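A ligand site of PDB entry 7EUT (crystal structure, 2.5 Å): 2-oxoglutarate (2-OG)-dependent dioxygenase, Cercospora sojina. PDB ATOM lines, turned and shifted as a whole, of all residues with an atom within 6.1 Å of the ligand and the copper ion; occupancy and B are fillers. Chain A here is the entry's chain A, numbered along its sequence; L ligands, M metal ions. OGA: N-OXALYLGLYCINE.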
ATOM      1  N   ARG A 140      27.037 -13.781   9.179  1.00  0.00           N
ATOM      2  CA  ARG A 140      26.710 -13.894  10.588  1.00  0.00           C
ATOM      3  C   ARG A 140      25.562 -14.879  10.770  1.00  0.00           C
ATOM      4  O   ARG A 140      24.598 -14.857   9.984  1.00  0.00           O
ATOM      5  CB  ARG A 140      26.331 -12.528  11.181  1.00  0.00           C
ATOM      6  CG  ARG A 140      27.272 -11.397  10.818  1.00  0.00           C
ATOM      7  CD  ARG A 140      26.789 -10.090  11.410  1.00  0.00           C
ATOM      8  NE  ARG A 140      27.663  -8.977  11.072  1.00  0.00           N
ATOM      9  CZ  ARG A 140      28.527  -8.424  11.919  1.00  0.00           C
ATOM     10  NH1 ARG A 140      28.651  -8.885  13.150  1.00  0.00           N
ATOM     11  NH2 ARG A 140      29.283  -7.400  11.522  1.00  0.00           N
ATOM     12  N   THR A 164      28.816 -13.600  15.390  1.00  0.00           N
ATOM     13  CA  THR A 164      27.571 -13.149  16.034  1.00  0.00           C
ATOM     14  C   THR A 164      27.144 -11.764  15.527  1.00  0.00           C
ATOM     15  O   THR A 164      27.861 -11.174  14.759  1.00  0.00           O
ATOM     16  CB  THR A 164      27.674 -13.094  17.557  1.00  0.00           C
ATOM     17  OG1 THR A 164      28.739 -12.199  17.795  1.00  0.00           O
ATOM     18  CG2 THR A 164      27.950 -14.434  18.203  1.00  0.00           C
ATOM     19  N   PRO A 165      25.976 -11.305  15.910  1.00  0.00           N
ATOM     20  CA  PRO A 165      25.509  -9.991  15.533  1.00  0.00           C
ATOM     21  C   PRO A 165      26.415  -8.855  16.026  1.00  0.00           C
ATOM     22  O   PRO A 165      26.969  -8.945  17.040  1.00  0.00           O
ATOM     23  CB  PRO A 165      24.215  -9.878  16.316  1.00  0.00           C
ATOM     24  CG  PRO A 165      23.617 -11.194  16.165  1.00  0.00           C
ATOM     25  CD  PRO A 165      24.800 -12.114  16.142  1.00  0.00           C
ATOM     26  N   GLY A 166      26.520  -7.810  15.212  1.00  0.00           N
ATOM     27  CA  GLY A 166      27.255  -6.589  15.553  1.00  0.00           C
ATOM     28  C   GLY A 166      26.402  -5.789  16.489  1.00  0.00           C
ATOM     29  O   GLY A 166      25.730  -4.907  16.047  1.00  0.00           O
ATOM     30  N   ARG A 167      26.469  -6.142  17.755  1.00  0.00           N
ATOM     31  CA  ARG A 167      25.591  -5.560  18.773  1.00  0.00           C
ATOM     32  C   ARG A 167      26.221  -4.333  19.440  1.00  0.00           C
ATOM     33  O   ARG A 167      26.314  -4.247  20.669  1.00  0.00           O
ATOM     34  CB  ARG A 167      25.250  -6.614  19.808  1.00  0.00           C
ATOM     35  CG  ARG A 167      23.844  -6.507  20.374  1.00  0.00           C
ATOM     36  CD  ARG A 167      23.613  -7.559  21.446  1.00  0.00           C
ATOM     37  NE  ARG A 167      22.586  -8.517  21.063  1.00  0.00           N
ATOM     38  CZ  ARG A 167      22.005  -9.360  21.912  1.00  0.00           C
ATOM     39  NH1 ARG A 167      22.346  -9.358  23.192  1.00  0.00           N
ATOM     40  NH2 ARG A 167      21.075 -10.205  21.487  1.00  0.00           N
ATOM     41  N   HIS A 170      28.179   1.595  15.505  1.00  0.00           N
ATOM     42  CA  HIS A 170      29.427   1.746  14.773  1.00  0.00           C
ATOM     43  C   HIS A 170      29.127   2.172  13.350  1.00  0.00           C
ATOM     44  O   HIS A 170      27.999   2.041  12.858  1.00  0.00           O
ATOM     45  CB  HIS A 170      30.236   0.438  14.763  1.00  0.00           C
ATOM     46  CG  HIS A 170      29.607  -0.654  13.952  1.00  0.00           C
ATOM     47  ND1 HIS A 170      28.490  -1.346  14.373  1.00  0.00           N
ATOM     48  CD2 HIS A 170      29.921  -1.161  12.740  1.00  0.00           C
ATOM     49  CE1 HIS A 170      28.154  -2.229  13.464  1.00  0.00           C
ATOM     50  NE2 HIS A 170      29.011  -2.138  12.455  1.00  0.00           N
ATOM     51  N   VAL A 171      30.157   2.696  12.697  1.00  0.00           N
ATOM     52  CA  VAL A 171      30.199   2.848  11.247  1.00  0.00           C
ATOM     53  C   VAL A 171      31.429   2.089  10.761  1.00  0.00           C
ATOM     54  O   VAL A 171      32.533   2.298  11.263  1.00  0.00           O
ATOM     55  CB  VAL A 171      30.258   4.325  10.824  1.00  0.00           C
ATOM     56  CG1 VAL A 171      30.143   4.451   9.301  1.00  0.00           C
ATOM     57  CG2 VAL A 171      29.160   5.122  11.507  1.00  0.00           C
ATOM     58  N   ASP A 172      31.217   1.198   9.784  1.00  0.00           N
ATOM     59  CA  ASP A 172      32.272   0.250   9.411  1.00  0.00           C
ATOM     60  C   ASP A 172      33.540   0.939   8.927  1.00  0.00           C
ATOM     61  O   ASP A 172      34.619   0.334   9.019  1.00  0.00           O
ATOM     62  CB  ASP A 172      31.744  -0.696   8.338  1.00  0.00           C
ATOM     63  CG  ASP A 172      30.768  -1.715   8.893  1.00  0.00           C
ATOM     64  OD1 ASP A 172      29.911  -1.328   9.724  1.00  0.00           O
ATOM     65  OD2 ASP A 172      30.852  -2.897   8.512  1.00  0.00           O
ATOM     66  N   ASN A 203      27.420  -1.020   2.544  1.00  0.00           N
ATOM     67  CA  ASN A 203      27.175  -2.424   2.828  1.00  0.00           C
ATOM     68  C   ASN A 203      25.758  -2.788   2.401  1.00  0.00           C
ATOM     69  O   ASN A 203      24.807  -2.044   2.655  1.00  0.00           O
ATOM     70  CB  ASN A 203      27.361  -2.728   4.310  1.00  0.00           C
ATOM     71  CG  ASN A 203      28.820  -2.861   4.708  1.00  0.00           C
ATOM     72  OD1 ASN A 203      29.716  -2.486   3.947  1.00  0.00           O
ATOM     73  ND2 ASN A 203      29.063  -3.400   5.891  1.00  0.00           N
ATOM     74  N   VAL A 204      25.630  -3.939   1.749  1.00  0.00           N
ATOM     75  CA  VAL A 204      24.337  -4.474   1.342  1.00  0.00           C
ATOM     76  C   VAL A 204      24.031  -5.649   2.273  1.00  0.00           C
ATOM     77  O   VAL A 204      24.696  -6.692   2.208  1.00  0.00           O
ATOM     78  CB  VAL A 204      24.324  -4.897  -0.127  1.00  0.00           C
ATOM     79  CG1 VAL A 204      22.979  -5.507  -0.493  1.00  0.00           C
ATOM     80  CG2 VAL A 204      24.642  -3.705  -1.021  1.00  0.00           C
ATOM     81  N   TRP A 205      23.035  -5.477   3.126  1.00  0.00           N
ATOM     82  CA  TRP A 205      22.722  -6.409   4.199  1.00  0.00           C
ATOM     83  C   TRP A 205      21.444  -7.168   3.861  1.00  0.00           C
ATOM     84  O   TRP A 205      20.373  -6.566   3.728  1.00  0.00           O
ATOM     85  CB  TRP A 205      22.561  -5.657   5.520  1.00  0.00           C
ATOM     86  CG  TRP A 205      22.468  -6.512   6.745  1.00  0.00           C
ATOM     87  CD1 TRP A 205      23.470  -6.813   7.610  1.00  0.00           C
ATOM     88  CD2 TRP A 205      21.284  -7.141   7.269  1.00  0.00           C
ATOM     89  NE1 TRP A 205      23.001  -7.604   8.630  1.00  0.00           N
ATOM     90  CE2 TRP A 205      21.659  -7.823   8.436  1.00  0.00           C
ATOM     91  CE3 TRP A 205      19.955  -7.204   6.845  1.00  0.00           C
ATOM     92  CZ2 TRP A 205      20.758  -8.556   9.201  1.00  0.00           C
ATOM     93  CZ3 TRP A 205      19.046  -7.929   7.601  1.00  0.00           C
ATOM     94  CH2 TRP A 205      19.456  -8.596   8.766  1.00  0.00           C
ATOM     95  N   GLU A 214      16.928 -10.507  16.487  1.00  0.00           N
ATOM     96  CA  GLU A 214      18.089  -9.627  16.347  1.00  0.00           C
ATOM     97  C   GLU A 214      18.096  -8.881  15.020  1.00  0.00           C
ATOM     98  O   GLU A 214      18.965  -9.116  14.169  1.00  0.00           O
ATOM     99  CB  GLU A 214      19.385 -10.433  16.502  1.00  0.00           C
ATOM    100  CG  GLU A 214      20.629  -9.582  16.730  1.00  0.00           C
ATOM    101  CD  GLU A 214      21.040  -9.514  18.192  1.00  0.00           C
ATOM    102  OE1 GLU A 214      20.696 -10.441  18.953  1.00  0.00           O
ATOM    103  OE2 GLU A 214      21.710  -8.523  18.571  1.00  0.00           O
ATOM    104  N   PRO A 215      17.149  -7.964  14.802  1.00  0.00           N
ATOM    105  CA  PRO A 215      17.167  -7.187  13.547  1.00  0.00           C
ATOM    106  C   PRO A 215      18.283  -6.146  13.519  1.00  0.00           C
ATOM    107  O   PRO A 215      19.070  -6.052  14.468  1.00  0.00           O
ATOM    108  CB  PRO A 215      15.787  -6.521  13.518  1.00  0.00           C
ATOM    109  CG  PRO A 215      15.376  -6.450  14.950  1.00  0.00           C
ATOM    110  CD  PRO A 215      15.982  -7.639  15.633  1.00  0.00           C
ATOM    111  N   LEU A 216      18.364  -5.375  12.444  1.00  0.00           N
ATOM    112  CA  LEU A 216      19.462  -4.435  12.220  1.00  0.00           C
ATOM    113  C   LEU A 216      18.919  -3.012  12.223  1.00  0.00           C
ATOM    114  O   LEU A 216      18.133  -2.646  11.345  1.00  0.00           O
ATOM    115  CB  LEU A 216      20.174  -4.737  10.902  1.00  0.00           C
ATOM    116  CG  LEU A 216      21.467  -3.956  10.697  1.00  0.00           C
ATOM    117  CD1 LEU A 216      22.468  -4.309  11.784  1.00  0.00           C
ATOM    118  CD2 LEU A 216      22.052  -4.225   9.320  1.00  0.00           C
ATOM    119  N   MET A 250      37.234   2.403  12.081  1.00  0.00           N
ATOM    120  CA  MET A 250      35.795   2.565  12.178  1.00  0.00           C
ATOM    121  C   MET A 250      35.459   3.888  12.863  1.00  0.00           C
ATOM    122  O   MET A 250      36.316   4.566  13.428  1.00  0.00           O
ATOM    123  CB  MET A 250      35.173   1.421  12.969  1.00  0.00           C
ATOM    124  CG  MET A 250      35.141   0.076  12.276  1.00  0.00           C
ATOM    125  SD  MET A 250      34.063  -1.056  13.183  1.00  0.00           S
ATOM    126  CE  MET A 250      33.676  -2.250  11.917  1.00  0.00           C
ATOM    127  N   ILE A 278      23.429   0.414   3.415  1.00  0.00           N
ATOM    128  CA  ILE A 278      23.938   1.238   4.517  1.00  0.00           C
ATOM    129  C   ILE A 278      25.175   1.973   4.030  1.00  0.00           C
ATOM    130  O   ILE A 278      26.225   1.344   3.828  1.00  0.00           O
ATOM    131  CB  ILE A 278      24.237   0.412   5.769  1.00  0.00           C
ATOM    132  CG1 ILE A 278      23.061  -0.506   6.113  1.00  0.00           C
ATOM    133  CG2 ILE A 278      24.569   1.328   6.943  1.00  0.00           C
ATOM    134  CD1 ILE A 278      23.221  -1.213   7.441  1.00  0.00           C
ATOM    135  N   MET A 280      28.364   3.720   4.486  1.00  0.00           N
ATOM    136  CA  MET A 280      29.387   3.924   5.509  1.00  0.00           C
ATOM    137  C   MET A 280      30.174   5.200   5.275  1.00  0.00           C
ATOM    138  O   MET A 280      30.593   5.859   6.245  1.00  0.00           O
ATOM    139  CB  MET A 280      30.350   2.737   5.525  1.00  0.00           C
ATOM    140  CG  MET A 280      29.682   1.391   5.623  1.00  0.00           C
ATOM    141  SD  MET A 280      28.676   1.277   7.104  1.00  0.00           S
ATOM    142  CE  MET A 280      27.922  -0.331   6.870  1.00  0.00           C
ATOM    143  N   HIS A 294      25.066   2.173  12.913  1.00  0.00           N
ATOM    144  CA  HIS A 294      24.132   1.060  12.862  1.00  0.00           C
ATOM    145  C   HIS A 294      24.541   0.041  13.916  1.00  0.00           C
ATOM    146  O   HIS A 294      25.678   0.028  14.389  1.00  0.00           O
ATOM    147  CB  HIS A 294      24.080   0.417  11.472  1.00  0.00           C
ATOM    148  CG  HIS A 294      25.425   0.019  10.945  1.00  0.00           C
ATOM    149  ND1 HIS A 294      26.363   0.939  10.538  1.00  0.00           N
ATOM    150  CD2 HIS A 294      25.980  -1.203  10.751  1.00  0.00           C
ATOM    151  CE1 HIS A 294      27.453   0.309  10.126  1.00  0.00           C
ATOM    152  NE2 HIS A 294      27.241  -0.989  10.240  1.00  0.00           N
ATOM    153  N   SER A 295      23.586  -0.817  14.270  1.00  0.00           N
ATOM    154  CA  SER A 295      23.816  -1.842  15.274  1.00  0.00           C
ATOM    155  C   SER A 295      22.653  -2.825  15.257  1.00  0.00           C
ATOM    156  O   SER A 295      21.501  -2.416  15.090  1.00  0.00           O
ATOM    157  CB  SER A 295      23.966  -1.231  16.680  1.00  0.00           C
ATOM    158  OG  SER A 295      23.754  -2.207  17.683  1.00  0.00           O
ATOM    159  N   SER A 296      22.975  -4.099  15.427  1.00  0.00           N
ATOM    160  CA  SER A 296      21.936  -5.085  15.696  1.00  0.00           C
ATOM    161  C   SER A 296      21.409  -4.892  17.114  1.00  0.00           C
ATOM    162  O   SER A 296      22.111  -4.402  17.999  1.00  0.00           O
ATOM    163  CB  SER A 296      22.480  -6.500  15.520  1.00  0.00           C
ATOM    164  OG  SER A 296      23.466  -6.788  16.503  1.00  0.00           O
ATOM    165  N   ARG A 307      19.205 -15.516  13.792  1.00  0.00           N
ATOM    166  CA  ARG A 307      19.257 -14.706  12.592  1.00  0.00           C
ATOM    167  C   ARG A 307      20.539 -14.985  11.808  1.00  0.00           C
ATOM    168  O   ARG A 307      21.629 -15.044  12.384  1.00  0.00           O
ATOM    169  CB  ARG A 307      19.184 -13.218  12.952  1.00  0.00           C
ATOM    170  CG  ARG A 307      18.918 -12.294  11.777  1.00  0.00           C
ATOM    171  CD  ARG A 307      20.146 -11.473  11.409  1.00  0.00           C
ATOM    172  NE  ARG A 307      20.484 -10.475  12.424  1.00  0.00           N
ATOM    173  CZ  ARG A 307      21.711 -10.017  12.636  1.00  0.00           C
ATOM    174  NH1 ARG A 307      22.729 -10.465  11.909  1.00  0.00           N
ATOM    175  NH2 ARG A 307      21.934  -9.108  13.578  1.00  0.00           N
ATOM    176  N   SER A 309      22.621 -13.818   8.129  1.00  0.00           N
ATOM    177  CA  SER A 309      22.671 -12.730   7.169  1.00  0.00           C
ATOM    178  C   SER A 309      24.060 -12.653   6.546  1.00  0.00           C
ATOM    179  O   SER A 309      25.031 -13.175   7.093  1.00  0.00           O
ATOM    180  CB  SER A 309      22.317 -11.385   7.812  1.00  0.00           C
ATOM    181  OG  SER A 309      23.331 -10.983   8.719  1.00  0.00           O
ATOM    182  N   GLU A 311      26.446  -9.400   4.877  1.00  0.00           N
ATOM    183  CA  GLU A 311      26.649  -7.999   4.548  1.00  0.00           C
ATOM    184  C   GLU A 311      27.812  -7.934   3.575  1.00  0.00           C
ATOM    185  O   GLU A 311      28.929  -8.349   3.902  1.00  0.00           O
ATOM    186  CB  GLU A 311      26.923  -7.163   5.804  1.00  0.00           C
ATOM    187  CG  GLU A 311      28.063  -7.686   6.669  1.00  0.00           C
ATOM    188  CD  GLU A 311      27.801  -7.554   8.146  1.00  0.00           C
ATOM    189  OE1 GLU A 311      28.730  -7.149   8.876  1.00  0.00           O
ATOM    190  OE2 GLU A 311      26.673  -7.867   8.593  1.00  0.00           O
HETATM  191  C1  OGA L   1      26.866  -4.358   8.749  1.00  0.00           C
HETATM  192  C2  OGA L   1      26.652  -4.763  10.203  1.00  0.00           C
HETATM  193  C4  OGA L   1      25.758  -6.317  11.936  1.00  0.00           C
HETATM  194  C5  OGA L   1      24.770  -7.477  12.067  1.00  0.00           C
HETATM  195  O1  OGA L   1      26.169  -4.890   7.848  1.00  0.00           O
HETATM  196  O2  OGA L   1      27.732  -3.485   8.463  1.00  0.00           O
HETATM  197  O2' OGA L   1      27.084  -4.074  11.071  1.00  0.00           O
HETATM  198  O3  OGA L   1      24.502  -7.943  13.204  1.00  0.00           O
HETATM  199  N1  OGA L   1      25.929  -5.974  10.538  1.00  0.00           N
HETATM  200  O4  OGA L   1      24.233  -7.967  11.048  1.00  0.00           O
HETATM  201 CU    CU M   1      28.550  -2.767  10.378  1.00  0.00          CU
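Three residues have an atom within 4 Å of the copper ion: His 170, Asp 172 and His 294.
Along chain A the residues within 4 Å of the copper ion span positions 170 to 294.
The nearest printed residue that does not touch the copper ion is Met 280 (4.3 Å).
The backbone carbonyl oxygen (O) of Gly 166 lies within hydrogen-bond range of the backbone NH (N) of Ser 296, 2.9 Å away.
The side-chain sulfur (SD) of Met 280 sits at hydrogen-bond distance from the backbone NH (N) of Asp 172, 3.7 Å away.
The side-chain hydroxyl (OG) of Ser 296 is in hydrogen-bond range of the backbone NH (N) of Arg 167.
The backbone NH (N) of Ile 278 lies within hydrogen-bond range of the backbone carbonyl oxygen (O) of Asn 203 (2.9 Å).
NE1 of Trp 205 is in hydrogen-bond range of OG of Ser 309 (3.4 Å).
The guanidinium group of Arg 307 sits at hydrogen-bond distance from the backbone carbonyl oxygen of Glu 214 (2.7 Å).
The backbone carbonyl oxygen of Arg 140 is in hydrogen-bond range of the backbone NH of Ser 309 (2.9 Å).
OG of Ser 296 is in hydrogen-bond range of OE2 of Glu 214 (3.2 Å).
CA of Pro 165 touches O3 of the ligand (3.3 Å).
Leu 216 touches the ligand.
CE of Met 280 touches O2 of the ligand, 3.5 Å away.
Ser 296 touches the ligand.
Ser 309 touches the ligand (OG to O4, 3.9 Å).
Hydrophobic or aromatic side chains within 4 Å of the ligand: Pro 165, His 170, Trp 205, Leu 216, Met 280 and His 294.
14 residues have an atom within 4 Å of the ligand: Arg 140, Pro 165, Gly 166, His 170, Asp 172, Asn 203, Trp 205, Leu 216, Met 280, His 294, Ser 296, Arg 307, Ser 309 and Glu 311.
The copper ion is bound by an oxygen (O2') of the ligand (2.1 Å), the side-chain carboxylate (OD1) of Asp 172 (2.1 Å), an oxygen (O2) of the ligand (2.2 Å), a ring nitrogen (NE2) of His 294 (2.2 Å) and a ring nitrogen (NE2) of His 170 (2.2 Å).
The copper ion has five donor atoms within binding distance.
N of Gly 166 is in hydrogen-bond range of O3 of the ligand.
OE2 of Glu 311 is in hydrogen-bond range of N1 of the ligand, 2.8 Å away.
The guanidinium group of Arg 140 lies within salt-bridge range of an oxygen (O4) of the ligand, 3.6 Å away.
ND2 of Asn 203 sits close to O2 of the ligand.
NE1 of Trp 205 sits at hydrogen-bond distance from O4 of the ligand.
NH2 of Arg 307 is in salt-bridge range of O3 of the ligand (2.8 Å).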
